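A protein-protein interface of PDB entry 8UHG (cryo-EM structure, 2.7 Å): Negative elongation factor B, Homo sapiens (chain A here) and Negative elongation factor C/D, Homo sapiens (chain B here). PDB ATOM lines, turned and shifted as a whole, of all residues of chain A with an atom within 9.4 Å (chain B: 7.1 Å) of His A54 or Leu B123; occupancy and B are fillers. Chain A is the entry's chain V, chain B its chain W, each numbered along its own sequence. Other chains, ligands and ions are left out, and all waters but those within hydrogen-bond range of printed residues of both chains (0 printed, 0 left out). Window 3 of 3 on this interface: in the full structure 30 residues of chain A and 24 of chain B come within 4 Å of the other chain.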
ATOM      1  N   ALA A  47      14.625  15.408 -19.993  1.00  0.00           N
ATOM      2  CA  ALA A  47      14.916  16.681 -19.340  1.00  0.00           C
ATOM      3  C   ALA A  47      14.172  17.856 -19.968  1.00  0.00           C
ATOM      4  O   ALA A  47      14.035  18.900 -19.319  1.00  0.00           O
ATOM      5  CB  ALA A  47      16.421  16.953 -19.378  1.00  0.00           C
ATOM      6  N   LEU A  48      13.714  17.721 -21.212  1.00  0.00           N
ATOM      7  CA  LEU A  48      13.031  18.816 -21.896  1.00  0.00           C
ATOM      8  C   LEU A  48      11.744  19.221 -21.186  1.00  0.00           C
ATOM      9  O   LEU A  48      11.552  20.428 -20.958  1.00  0.00           O
ATOM     10  CB  LEU A  48      12.784  18.430 -23.368  1.00  0.00           C
ATOM     11  CG  LEU A  48      13.862  18.397 -24.474  1.00  0.00           C
ATOM     12  CD1 LEU A  48      13.287  18.702 -25.844  1.00  0.00           C
ATOM     13  CD2 LEU A  48      15.050  19.293 -24.204  1.00  0.00           C
ATOM     14  N   PRO A  49      10.831  18.307 -20.815  1.00  0.00           N
ATOM     15  CA  PRO A  49       9.698  18.732 -19.966  1.00  0.00           C
ATOM     16  C   PRO A  49      10.107  19.325 -18.626  1.00  0.00           C
ATOM     17  O   PRO A  49       9.502  20.308 -18.176  1.00  0.00           O
ATOM     18  CB  PRO A  49       8.903  17.432 -19.769  1.00  0.00           C
ATOM     19  CG  PRO A  49       9.241  16.598 -20.910  1.00  0.00           C
ATOM     20  CD  PRO A  49      10.628  16.941 -21.337  1.00  0.00           C
ATOM     21  N   PHE A  50      11.120  18.753 -17.970  1.00  0.00           N
ATOM     22  CA  PHE A  50      11.498  19.222 -16.639  1.00  0.00           C
ATOM     23  C   PHE A  50      12.045  20.642 -16.690  1.00  0.00           C
ATOM     24  O   PHE A  50      11.666  21.494 -15.882  1.00  0.00           O
ATOM     25  CB  PHE A  50      12.527  18.281 -16.013  1.00  0.00           C
ATOM     26  CG  PHE A  50      13.222  18.870 -14.819  1.00  0.00           C
ATOM     27  CD1 PHE A  50      12.516  19.147 -13.661  1.00  0.00           C
ATOM     28  CD2 PHE A  50      14.578  19.152 -14.855  1.00  0.00           C
ATOM     29  CE1 PHE A  50      13.147  19.694 -12.562  1.00  0.00           C
ATOM     30  CE2 PHE A  50      15.216  19.697 -13.756  1.00  0.00           C
ATOM     31  CZ  PHE A  50      14.498  19.968 -12.608  1.00  0.00           C
ATOM     32  N   LEU A  51      12.956  20.910 -17.624  1.00  0.00           N
ATOM     33  CA  LEU A  51      13.472  22.265 -17.774  1.00  0.00           C
ATOM     34  C   LEU A  51      12.396  23.202 -18.313  1.00  0.00           C
ATOM     35  O   LEU A  51      12.417  24.408 -18.037  1.00  0.00           O
ATOM     36  CB  LEU A  51      14.703  22.251 -18.678  1.00  0.00           C
ATOM     37  CG  LEU A  51      15.401  23.557 -19.062  1.00  0.00           C
ATOM     38  CD1 LEU A  51      16.127  24.197 -17.890  1.00  0.00           C
ATOM     39  CD2 LEU A  51      16.368  23.239 -20.174  1.00  0.00           C
ATOM     40  N   ASP A  52      11.460  22.672 -19.106  1.00  0.00           N
ATOM     41  CA  ASP A  52      10.327  23.476 -19.559  1.00  0.00           C
ATOM     42  C   ASP A  52       9.464  23.946 -18.392  1.00  0.00           C
ATOM     43  O   ASP A  52       8.882  25.036 -18.441  1.00  0.00           O
ATOM     44  CB  ASP A  52       9.482  22.677 -20.556  1.00  0.00           C
ATOM     45  CG  ASP A  52       9.975  22.812 -21.990  1.00  0.00           C
ATOM     46  OD1 ASP A  52      10.305  23.939 -22.418  1.00  0.00           O
ATOM     47  OD2 ASP A  52      10.031  21.789 -22.700  1.00  0.00           O
ATOM     48  N   LEU A  53       9.332  23.117 -17.353  1.00  0.00           N
ATOM     49  CA  LEU A  53       8.533  23.496 -16.185  1.00  0.00           C
ATOM     50  C   LEU A  53       9.042  24.775 -15.519  1.00  0.00           C
ATOM     51  O   LEU A  53       8.254  25.502 -14.903  1.00  0.00           O
ATOM     52  CB  LEU A  53       8.517  22.346 -15.170  1.00  0.00           C
ATOM     53  CG  LEU A  53       7.806  22.479 -13.808  1.00  0.00           C
ATOM     54  CD1 LEU A  53       6.343  22.083 -13.897  1.00  0.00           C
ATOM     55  CD2 LEU A  53       8.531  21.644 -12.758  1.00  0.00           C
ATOM     56  N   HIS A  54      10.342  25.065 -15.618  1.00  0.00           N
ATOM     57  CA  HIS A  54      10.931  26.196 -14.903  1.00  0.00           C
ATOM     58  C   HIS A  54      10.494  27.559 -15.429  1.00  0.00           C
ATOM     59  O   HIS A  54      10.756  28.564 -14.757  1.00  0.00           O
ATOM     60  CB  HIS A  54      12.458  26.124 -14.976  1.00  0.00           C
ATOM     61  CG  HIS A  54      13.049  24.942 -14.274  1.00  0.00           C
ATOM     62  ND1 HIS A  54      14.372  24.585 -14.409  1.00  0.00           N
ATOM     63  CD2 HIS A  54      12.501  24.040 -13.425  1.00  0.00           C
ATOM     64  CE1 HIS A  54      14.615  23.513 -13.679  1.00  0.00           C
ATOM     65  NE2 HIS A  54      13.496  23.161 -13.071  1.00  0.00           N
ATOM     66  N   GLY A  55       9.843  27.625 -16.586  1.00  0.00           N
ATOM     67  CA  GLY A  55       9.704  28.869 -17.316  1.00  0.00           C
ATOM     68  C   GLY A  55      10.815  29.135 -18.311  1.00  0.00           C
ATOM     69  O   GLY A  55      10.851  30.225 -18.893  1.00  0.00           O
ATOM     70  N   THR A  56      11.715  28.164 -18.526  1.00  0.00           N
ATOM     71  CA  THR A  56      12.790  28.258 -19.502  1.00  0.00           C
ATOM     72  C   THR A  56      12.424  27.403 -20.710  1.00  0.00           C
ATOM     73  O   THR A  56      12.366  26.172 -20.573  1.00  0.00           O
ATOM     74  CB  THR A  56      14.102  27.769 -18.894  1.00  0.00           C
ATOM     75  OG1 THR A  56      14.402  28.525 -17.716  1.00  0.00           O
ATOM     76  CG2 THR A  56      15.247  27.907 -19.887  1.00  0.00           C
ATOM     77  N   PRO A  57      12.171  27.965 -21.895  1.00  0.00           N
ATOM     78  CA  PRO A  57      11.859  27.105 -23.040  1.00  0.00           C
ATOM     79  C   PRO A  57      13.089  26.358 -23.538  1.00  0.00           C
ATOM     80  O   PRO A  57      14.233  26.701 -23.229  1.00  0.00           O
ATOM     81  CB  PRO A  57      11.327  28.086 -24.088  1.00  0.00           C
ATOM     82  CG  PRO A  57      12.059  29.334 -23.803  1.00  0.00           C
ATOM     83  CD  PRO A  57      12.150  29.387 -22.295  1.00  0.00           C
ATOM     84  N   ARG A  58      12.815  25.298 -24.304  1.00  0.00           N
ATOM     85  CA  ARG A  58      13.860  24.417 -24.831  1.00  0.00           C
ATOM     86  C   ARG A  58      14.856  25.194 -25.690  1.00  0.00           C
ATOM     87  O   ARG A  58      16.081  24.970 -25.646  1.00  0.00           O
ATOM     88  CB  ARG A  58      13.203  23.298 -25.655  1.00  0.00           C
ATOM     89  CG  ARG A  58      12.154  22.428 -24.911  1.00  0.00           C
ATOM     90  CD  ARG A  58      11.252  21.634 -25.873  1.00  0.00           C
ATOM     91  NE  ARG A  58      10.581  20.520 -25.212  1.00  0.00           N
ATOM     92  CZ  ARG A  58       9.931  19.539 -25.829  1.00  0.00           C
ATOM     93  NH1 ARG A  58       9.830  19.488 -27.150  1.00  0.00           N
ATOM     94  NH2 ARG A  58       9.386  18.568 -25.103  1.00  0.00           N
ATOM     95  N   GLU A  60      16.013  28.001 -25.184  1.00  0.00           N
ATOM     96  CA  GLU A  60      16.928  28.872 -24.446  1.00  0.00           C
ATOM     97  C   GLU A  60      18.262  28.180 -24.180  1.00  0.00           C
ATOM     98  O   GLU A  60      19.336  28.734 -24.477  1.00  0.00           O
ATOM     99  CB  GLU A  60      16.279  29.325 -23.138  1.00  0.00           C
ATOM    100  CG  GLU A  60      17.022  30.467 -22.446  1.00  0.00           C
ATOM    101  CD  GLU A  60      16.191  31.160 -21.381  1.00  0.00           C
ATOM    102  OE1 GLU A  60      15.098  31.667 -21.711  1.00  0.00           O
ATOM    103  OE2 GLU A  60      16.629  31.192 -20.211  1.00  0.00           O
ATOM    104  N   TYR B  56       9.128  31.667 -27.477  1.00  0.00           N
ATOM    105  CA  TYR B  56       8.613  31.015 -26.272  1.00  0.00           C
ATOM    106  C   TYR B  56       7.746  29.786 -26.558  1.00  0.00           C
ATOM    107  O   TYR B  56       7.328  29.120 -25.605  1.00  0.00           O
ATOM    108  CB  TYR B  56       7.810  32.031 -25.444  1.00  0.00           C
ATOM    109  CG  TYR B  56       7.517  31.662 -23.993  1.00  0.00           C
ATOM    110  CD1 TYR B  56       8.437  31.920 -22.983  1.00  0.00           C
ATOM    111  CD2 TYR B  56       6.302  31.094 -23.632  1.00  0.00           C
ATOM    112  CE1 TYR B  56       8.161  31.595 -21.661  1.00  0.00           C
ATOM    113  CE2 TYR B  56       6.021  30.760 -22.323  1.00  0.00           C
ATOM    114  CZ  TYR B  56       6.947  31.021 -21.339  1.00  0.00           C
ATOM    115  OH  TYR B  56       6.661  30.692 -20.034  1.00  0.00           O
ATOM    116  N   GLU B  59       7.487  25.918 -24.605  1.00  0.00           N
ATOM    117  CA  GLU B  59       7.332  25.705 -23.167  1.00  0.00           C
ATOM    118  C   GLU B  59       6.216  24.717 -22.844  1.00  0.00           C
ATOM    119  O   GLU B  59       5.705  24.029 -23.728  1.00  0.00           O
ATOM    120  CB  GLU B  59       7.065  27.045 -22.468  1.00  0.00           C
ATOM    121  CG  GLU B  59       8.303  27.745 -21.959  1.00  0.00           C
ATOM    122  CD  GLU B  59       8.425  27.682 -20.464  1.00  0.00           C
ATOM    123  OE1 GLU B  59       7.504  28.158 -19.771  1.00  0.00           O
ATOM    124  OE2 GLU B  59       9.442  27.142 -19.989  1.00  0.00           O
ATOM    125  N   SER B  61       4.477  25.825 -19.438  1.00  0.00           N
ATOM    126  CA  SER B  61       3.615  26.918 -18.999  1.00  0.00           C
ATOM    127  C   SER B  61       2.982  27.663 -20.174  1.00  0.00           C
ATOM    128  O   SER B  61       2.055  28.449 -19.975  1.00  0.00           O
ATOM    129  CB  SER B  61       4.402  27.897 -18.127  1.00  0.00           C
ATOM    130  OG  SER B  61       5.448  28.502 -18.862  1.00  0.00           O
ATOM    131  N   GLU B 116      26.399  20.069 -19.440  1.00  0.00           N
ATOM    132  CA  GLU B 116      26.068  19.760 -18.054  1.00  0.00           C
ATOM    133  C   GLU B 116      26.544  20.858 -17.115  1.00  0.00           C
ATOM    134  O   GLU B 116      25.813  21.257 -16.204  1.00  0.00           O
ATOM    135  CB  GLU B 116      26.675  18.414 -17.657  1.00  0.00           C
ATOM    136  CG  GLU B 116      25.982  17.216 -18.287  1.00  0.00           C
ATOM    137  CD  GLU B 116      26.700  15.910 -18.004  1.00  0.00           C
ATOM    138  OE1 GLU B 116      27.338  15.799 -16.936  1.00  0.00           O
ATOM    139  OE2 GLU B 116      26.631  14.997 -18.854  1.00  0.00           O
ATOM    140  N   ASN B 117      27.760  21.369 -17.326  1.00  0.00           N
ATOM    141  CA  ASN B 117      28.272  22.447 -16.486  1.00  0.00           C
ATOM    142  C   ASN B 117      27.421  23.701 -16.625  1.00  0.00           C
ATOM    143  O   ASN B 117      27.075  24.337 -15.624  1.00  0.00           O
ATOM    144  CB  ASN B 117      29.729  22.745 -16.845  1.00  0.00           C
ATOM    145  CG  ASN B 117      30.670  21.631 -16.437  1.00  0.00           C
ATOM    146  OD1 ASN B 117      30.252  20.491 -16.232  1.00  0.00           O
ATOM    147  ND2 ASN B 117      31.953  21.955 -16.318  1.00  0.00           N
ATOM    148  N   HIS B 118      27.059  24.059 -17.863  1.00  0.00           N
ATOM    149  CA  HIS B 118      26.227  25.240 -18.085  1.00  0.00           C
ATOM    150  C   HIS B 118      24.882  25.111 -17.381  1.00  0.00           C
ATOM    151  O   HIS B 118      24.480  25.998 -16.614  1.00  0.00           O
ATOM    152  CB  HIS B 118      26.019  25.465 -19.585  1.00  0.00           C
ATOM    153  CG  HIS B 118      27.109  26.256 -20.238  1.00  0.00           C
ATOM    154  ND1 HIS B 118      28.045  25.687 -21.073  1.00  0.00           N
ATOM    155  CD2 HIS B 118      27.409  27.575 -20.180  1.00  0.00           C
ATOM    156  CE1 HIS B 118      28.876  26.622 -21.501  1.00  0.00           C
ATOM    157  NE2 HIS B 118      28.511  27.776 -20.973  1.00  0.00           N
ATOM    158  N   LEU B 119      24.179  23.999 -17.609  1.00  0.00           N
ATOM    159  CA  LEU B 119      22.842  23.856 -17.044  1.00  0.00           C
ATOM    160  C   LEU B 119      22.892  23.726 -15.524  1.00  0.00           C
ATOM    161  O   LEU B 119      22.053  24.303 -14.823  1.00  0.00           O
ATOM    162  CB  LEU B 119      22.134  22.656 -17.679  1.00  0.00           C
ATOM    163  CG  LEU B 119      20.601  22.718 -17.745  1.00  0.00           C
ATOM    164  CD1 LEU B 119      20.077  21.945 -18.946  1.00  0.00           C
ATOM    165  CD2 LEU B 119      19.969  22.195 -16.467  1.00  0.00           C
ATOM    166  N   LYS B 120      23.876  22.994 -14.992  1.00  0.00           N
ATOM    167  CA  LYS B 120      24.008  22.852 -13.546  1.00  0.00           C
ATOM    168  C   LYS B 120      24.330  24.188 -12.883  1.00  0.00           C
ATOM    169  O   LYS B 120      23.792  24.501 -11.813  1.00  0.00           O
ATOM    170  CB  LYS B 120      25.093  21.821 -13.235  1.00  0.00           C
ATOM    171  CG  LYS B 120      25.254  21.469 -11.756  1.00  0.00           C
ATOM    172  CD  LYS B 120      26.327  20.406 -11.542  1.00  0.00           C
ATOM    173  CE  LYS B 120      27.732  20.954 -11.771  1.00  0.00           C
ATOM    174  NZ  LYS B 120      28.790  19.979 -11.392  1.00  0.00           N
ATOM    175  N   SER B 121      25.217  24.981 -13.491  1.00  0.00           N
ATOM    176  CA  SER B 121      25.520  26.297 -12.946  1.00  0.00           C
ATOM    177  C   SER B 121      24.294  27.197 -12.988  1.00  0.00           C
ATOM    178  O   SER B 121      24.047  27.962 -12.049  1.00  0.00           O
ATOM    179  CB  SER B 121      26.680  26.929 -13.714  1.00  0.00           C
ATOM    180  OG  SER B 121      27.842  26.123 -13.635  1.00  0.00           O
ATOM    181  N   LEU B 122      23.513  27.119 -14.070  1.00  0.00           N
ATOM    182  CA  LEU B 122      22.275  27.890 -14.139  1.00  0.00           C
ATOM    183  C   LEU B 122      21.308  27.474 -13.038  1.00  0.00           C
ATOM    184  O   LEU B 122      20.645  28.323 -12.433  1.00  0.00           O
ATOM    185  CB  LEU B 122      21.623  27.722 -15.512  1.00  0.00           C
ATOM    186  CG  LEU B 122      22.317  28.384 -16.707  1.00  0.00           C
ATOM    187  CD1 LEU B 122      21.760  27.823 -18.008  1.00  0.00           C
ATOM    188  CD2 LEU B 122      22.167  29.899 -16.680  1.00  0.00           C
ATOM    189  N   LEU B 123      21.215  26.170 -12.765  1.00  0.00           N
ATOM    190  CA  LEU B 123      20.365  25.695 -11.677  1.00  0.00           C
ATOM    191  C   LEU B 123      20.827  26.247 -10.336  1.00  0.00           C
ATOM    192  O   LEU B 123      20.021  26.763  -9.554  1.00  0.00           O
ATOM    193  CB  LEU B 123      20.366  24.168 -11.634  1.00  0.00           C
ATOM    194  CG  LEU B 123      19.675  23.422 -12.778  1.00  0.00           C
ATOM    195  CD1 LEU B 123      20.056  21.943 -12.793  1.00  0.00           C
ATOM    196  CD2 LEU B 123      18.162  23.573 -12.686  1.00  0.00           C
ATOM    197  N   ILE B 124      22.130  26.146 -10.055  1.00  0.00           N
ATOM    198  CA  ILE B 124      22.650  26.565  -8.753  1.00  0.00           C
ATOM    199  C   ILE B 124      22.471  28.067  -8.571  1.00  0.00           C
ATOM    200  O   ILE B 124      22.102  28.538  -7.488  1.00  0.00           O
ATOM    201  CB  ILE B 124      24.128  26.156  -8.590  1.00  0.00           C
ATOM    202  CG1 ILE B 124      24.301  24.631  -8.640  1.00  0.00           C
ATOM    203  CG2 ILE B 124      24.672  26.675  -7.255  1.00  0.00           C
ATOM    204  CD1 ILE B 124      25.704  24.184  -9.012  1.00  0.00           C
ATOM    205  N   LYS B 125      22.736  28.843  -9.625  1.00  0.00           N
ATOM    206  CA  LYS B 125      22.516  30.283  -9.561  1.00  0.00           C
ATOM    207  C   LYS B 125      21.038  30.623  -9.416  1.00  0.00           C
ATOM    208  O   LYS B 125      20.697  31.613  -8.759  1.00  0.00           O
ATOM    209  CB  LYS B 125      23.096  30.950 -10.809  1.00  0.00           C
ATOM    210  CG  LYS B 125      24.612  31.097 -10.784  1.00  0.00           C
ATOM    211  CD  LYS B 125      25.241  31.044 -12.180  1.00  0.00           C
ATOM    212  CE  LYS B 125      24.644  32.053 -13.157  1.00  0.00           C
ATOM    213  NZ  LYS B 125      24.644  33.443 -12.629  1.00  0.00           N
ATOM    214  N   HIS B 126      20.154  29.813 -10.008  1.00  0.00           N
ATOM    215  CA  HIS B 126      18.717  30.062 -10.022  1.00  0.00           C
ATOM    216  C   HIS B 126      17.928  29.086  -9.155  1.00  0.00           C
ATOM    217  O   HIS B 126      16.693  29.086  -9.221  1.00  0.00           O
ATOM    218  CB  HIS B 126      18.197  30.005 -11.459  1.00  0.00           C
ATOM    219  CG  HIS B 126      18.964  30.867 -12.412  1.00  0.00           C
ATOM    220  ND1 HIS B 126      19.429  30.404 -13.624  1.00  0.00           N
ATOM    221  CD2 HIS B 126      19.350  32.163 -12.332  1.00  0.00           C
ATOM    222  CE1 HIS B 126      20.067  31.377 -14.250  1.00  0.00           C
ATOM    223  NE2 HIS B 126      20.034  32.454 -13.487  1.00  0.00           N
ATOM    224  N   PHE B 127      18.591  28.246  -8.360  1.00  0.00           N
ATOM    225  CA  PHE B 127      17.860  27.381  -7.443  1.00  0.00           C
ATOM    226  C   PHE B 127      17.136  28.224  -6.404  1.00  0.00           C
ATOM    227  O   PHE B 127      17.704  29.170  -5.850  1.00  0.00           O
ATOM    228  CB  PHE B 127      18.799  26.392  -6.749  1.00  0.00           C
ATOM    229  CG  PHE B 127      18.114  25.525  -5.722  1.00  0.00           C
ATOM    230  CD1 PHE B 127      17.425  24.386  -6.109  1.00  0.00           C
ATOM    231  CD2 PHE B 127      18.163  25.846  -4.373  1.00  0.00           C
ATOM    232  CE1 PHE B 127      16.795  23.588  -5.173  1.00  0.00           C
ATOM    233  CE2 PHE B 127      17.535  25.049  -3.434  1.00  0.00           C
ATOM    234  CZ  PHE B 127      16.851  23.921  -3.835  1.00  0.00           C
ATOM    235  N   ASP B 128      15.883  27.869  -6.149  1.00  0.00           N
ATOM    236  CA  ASP B 128      15.049  28.517  -5.137  1.00  0.00           C
ATOM    237  C   ASP B 128      14.666  27.468  -4.094  1.00  0.00           C
ATOM    238  O   ASP B 128      13.977  26.492  -4.449  1.00  0.00           O
ATOM    239  CB  ASP B 128      13.803  29.116  -5.784  1.00  0.00           C
ATOM    240  CG  ASP B 128      13.070  30.078  -4.865  1.00  0.00           C
ATOM    241  OD1 ASP B 128      13.432  30.175  -3.675  1.00  0.00           O
ATOM    242  OD2 ASP B 128      12.130  30.749  -5.341  1.00  0.00           O
ATOM    243  N   TRP B 145      11.726  12.397 -12.564  1.00  0.00           N
ATOM    244  CA  TRP B 145      12.836  13.240 -13.007  1.00  0.00           C
ATOM    245  C   TRP B 145      13.946  13.294 -11.959  1.00  0.00           C
ATOM    246  O   TRP B 145      15.131  13.287 -12.309  1.00  0.00           O
ATOM    247  CB  TRP B 145      12.359  14.655 -13.375  1.00  0.00           C
ATOM    248  CG  TRP B 145      11.451  15.368 -12.401  1.00  0.00           C
ATOM    249  CD1 TRP B 145      10.090  15.320 -12.370  1.00  0.00           C
ATOM    250  CD2 TRP B 145      11.842  16.263 -11.351  1.00  0.00           C
ATOM    251  NE1 TRP B 145       9.607  16.111 -11.358  1.00  0.00           N
ATOM    252  CE2 TRP B 145      10.664  16.703 -10.718  1.00  0.00           C
ATOM    253  CE3 TRP B 145      13.071  16.728 -10.880  1.00  0.00           C
ATOM    254  CZ2 TRP B 145      10.681  17.584  -9.641  1.00  0.00           C
ATOM    255  CZ3 TRP B 145      13.087  17.602  -9.811  1.00  0.00           C
ATOM    256  CH2 TRP B 145      11.900  18.020  -9.203  1.00  0.00           C
ATOM    257  N   MET B 149      17.680  11.938 -12.563  1.00  0.00           N
ATOM    258  CA  MET B 149      18.834  12.803 -12.350  1.00  0.00           C
ATOM    259  C   MET B 149      19.862  12.140 -11.442  1.00  0.00           C
ATOM    260  O   MET B 149      21.070  12.245 -11.685  1.00  0.00           O
ATOM    261  CB  MET B 149      18.378  14.134 -11.757  1.00  0.00           C
ATOM    262  CG  MET B 149      17.704  15.046 -12.765  1.00  0.00           C
ATOM    263  SD  MET B 149      16.380  16.109 -12.130  1.00  0.00           S
ATOM    264  CE  MET B 149      16.984  16.813 -10.585  1.00  0.00           C
ATOM    265  N   TRP B 155      24.605  15.397 -11.033  1.00  0.00           N
ATOM    266  CA  TRP B 155      23.357  15.795 -10.392  1.00  0.00           C
ATOM    267  C   TRP B 155      23.280  15.300  -8.953  1.00  0.00           C
ATOM    268  O   TRP B 155      22.653  15.945  -8.105  1.00  0.00           O
ATOM    269  CB  TRP B 155      22.172  15.270 -11.192  1.00  0.00           C
ATOM    270  CG  TRP B 155      21.944  15.973 -12.495  1.00  0.00           C
ATOM    271  CD1 TRP B 155      22.624  15.779 -13.662  1.00  0.00           C
ATOM    272  CD2 TRP B 155      20.956  16.973 -12.768  1.00  0.00           C
ATOM    273  NE1 TRP B 155      22.123  16.597 -14.644  1.00  0.00           N
ATOM    274  CE2 TRP B 155      21.098  17.341 -14.121  1.00  0.00           C
ATOM    275  CE3 TRP B 155      19.968  17.596 -12.001  1.00  0.00           C
ATOM    276  CZ2 TRP B 155      20.289  18.301 -14.721  1.00  0.00           C
ATOM    277  CZ3 TRP B 155      19.167  18.547 -12.600  1.00  0.00           C
ATOM    278  CH2 TRP B 155      19.327  18.885 -13.947  1.00  0.00           C
ATOM    279  N   LEU B 158      25.134  17.806  -7.235  1.00  0.00           N
ATOM    280  CA  LEU B 158      24.269  18.980  -7.170  1.00  0.00           C
ATOM    281  C   LEU B 158      23.322  18.886  -5.980  1.00  0.00           C
ATOM    282  O   LEU B 158      23.174  19.842  -5.213  1.00  0.00           O
ATOM    283  CB  LEU B 158      23.483  19.131  -8.478  1.00  0.00           C
ATOM    284  CG  LEU B 158      22.423  20.234  -8.588  1.00  0.00           C
ATOM    285  CD1 LEU B 158      23.049  21.603  -8.442  1.00  0.00           C
ATOM    286  CD2 LEU B 158      21.681  20.119  -9.910  1.00  0.00           C
ATOM    287  N   LEU B 162      23.163  21.211  -2.665  1.00  0.00           N
ATOM    288  CA  LEU B 162      21.892  21.866  -2.375  1.00  0.00           C
ATOM    289  C   LEU B 162      21.427  21.562  -0.956  1.00  0.00           C
ATOM    290  O   LEU B 162      21.003  22.465  -0.225  1.00  0.00           O
ATOM    291  CB  LEU B 162      20.828  21.425  -3.386  1.00  0.00           C
ATOM    292  CG  LEU B 162      20.840  21.993  -4.811  1.00  0.00           C
ATOM    293  CD1 LEU B 162      19.734  21.338  -5.632  1.00  0.00           C
ATOM    294  CD2 LEU B 162      20.689  23.496  -4.809  1.00  0.00           C
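The side-chain carboxylate (OE1) of Glu B59 sits at hydrogen-bond distance from the side-chain hydroxyl (OH) of Tyr B56 (2.7 Å).
O of Leu A48 sits close to OD2 of Asp A52, 2.7 Å away.
The side-chain carboxylate (OD2) of Asp A52 lies within salt-bridge range of the guanidinium group (NE) of Arg A58 (2.9 Å).
Hydrophobic or aromatic side chains of chain A within 4 Å of the printed part of chain B: Phe A50, His A54 and Pro A57.
Hydrophobic or aromatic side chains of chain B that line the printed part of chain A: Leu B123 and Trp B145.
Among the printed residues, 6 pairs touch across the chains.
Among the printed residues, no Asp or Glu carboxylate lies within 4 Å of a Lys or Arg side-chain nitrogen of the other chain.
The side-chain carboxylate (OE2) of Glu B59 sits at hydrogen-bond distance from the backbone NH (N) of Thr A56.
The side-chain carboxylate of Glu B59 lies close to the backbone nitrogen of Pro A57, at 3.4 Å.
The backbone NH (N) of Gly A55 lies close to the side-chain carboxylate (OE2) of Glu B59, at 3.5 Å.
The backbone carbonyl oxygen of Asp A52 sits close to the side-chain carboxylate of Glu B59.
Printed residues of chain B within 4 Å of Phe A50: Trp B145 (3.4 Å).
Of the printed residues of chain B, Asp A52 touches Glu B59.
Of the printed residues of chain A, Glu B59 touches Asp A52 (2.7 Å), Gly A55 (2.9 Å), Thr A56 (2.9 Å) and Pro A57 (3.4 Å).
Leu B123 touches just one residue of chain A: His A54 (3.7 Å).
His B126 touches none of the printed residues of chain A.
The nearest residue of chain A that does not touch Leu B123 is Phe A50 (5.0 Å).
The nearest printed residue of chain B that does not touch Pro A57 is Tyr B56 (4.4 Å).
CE1 of Phe A50 touches CE3 of Trp B145 (3.4 Å).
Leu B123 touches His A54 (CD2 to CE1, 3.7 Å).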
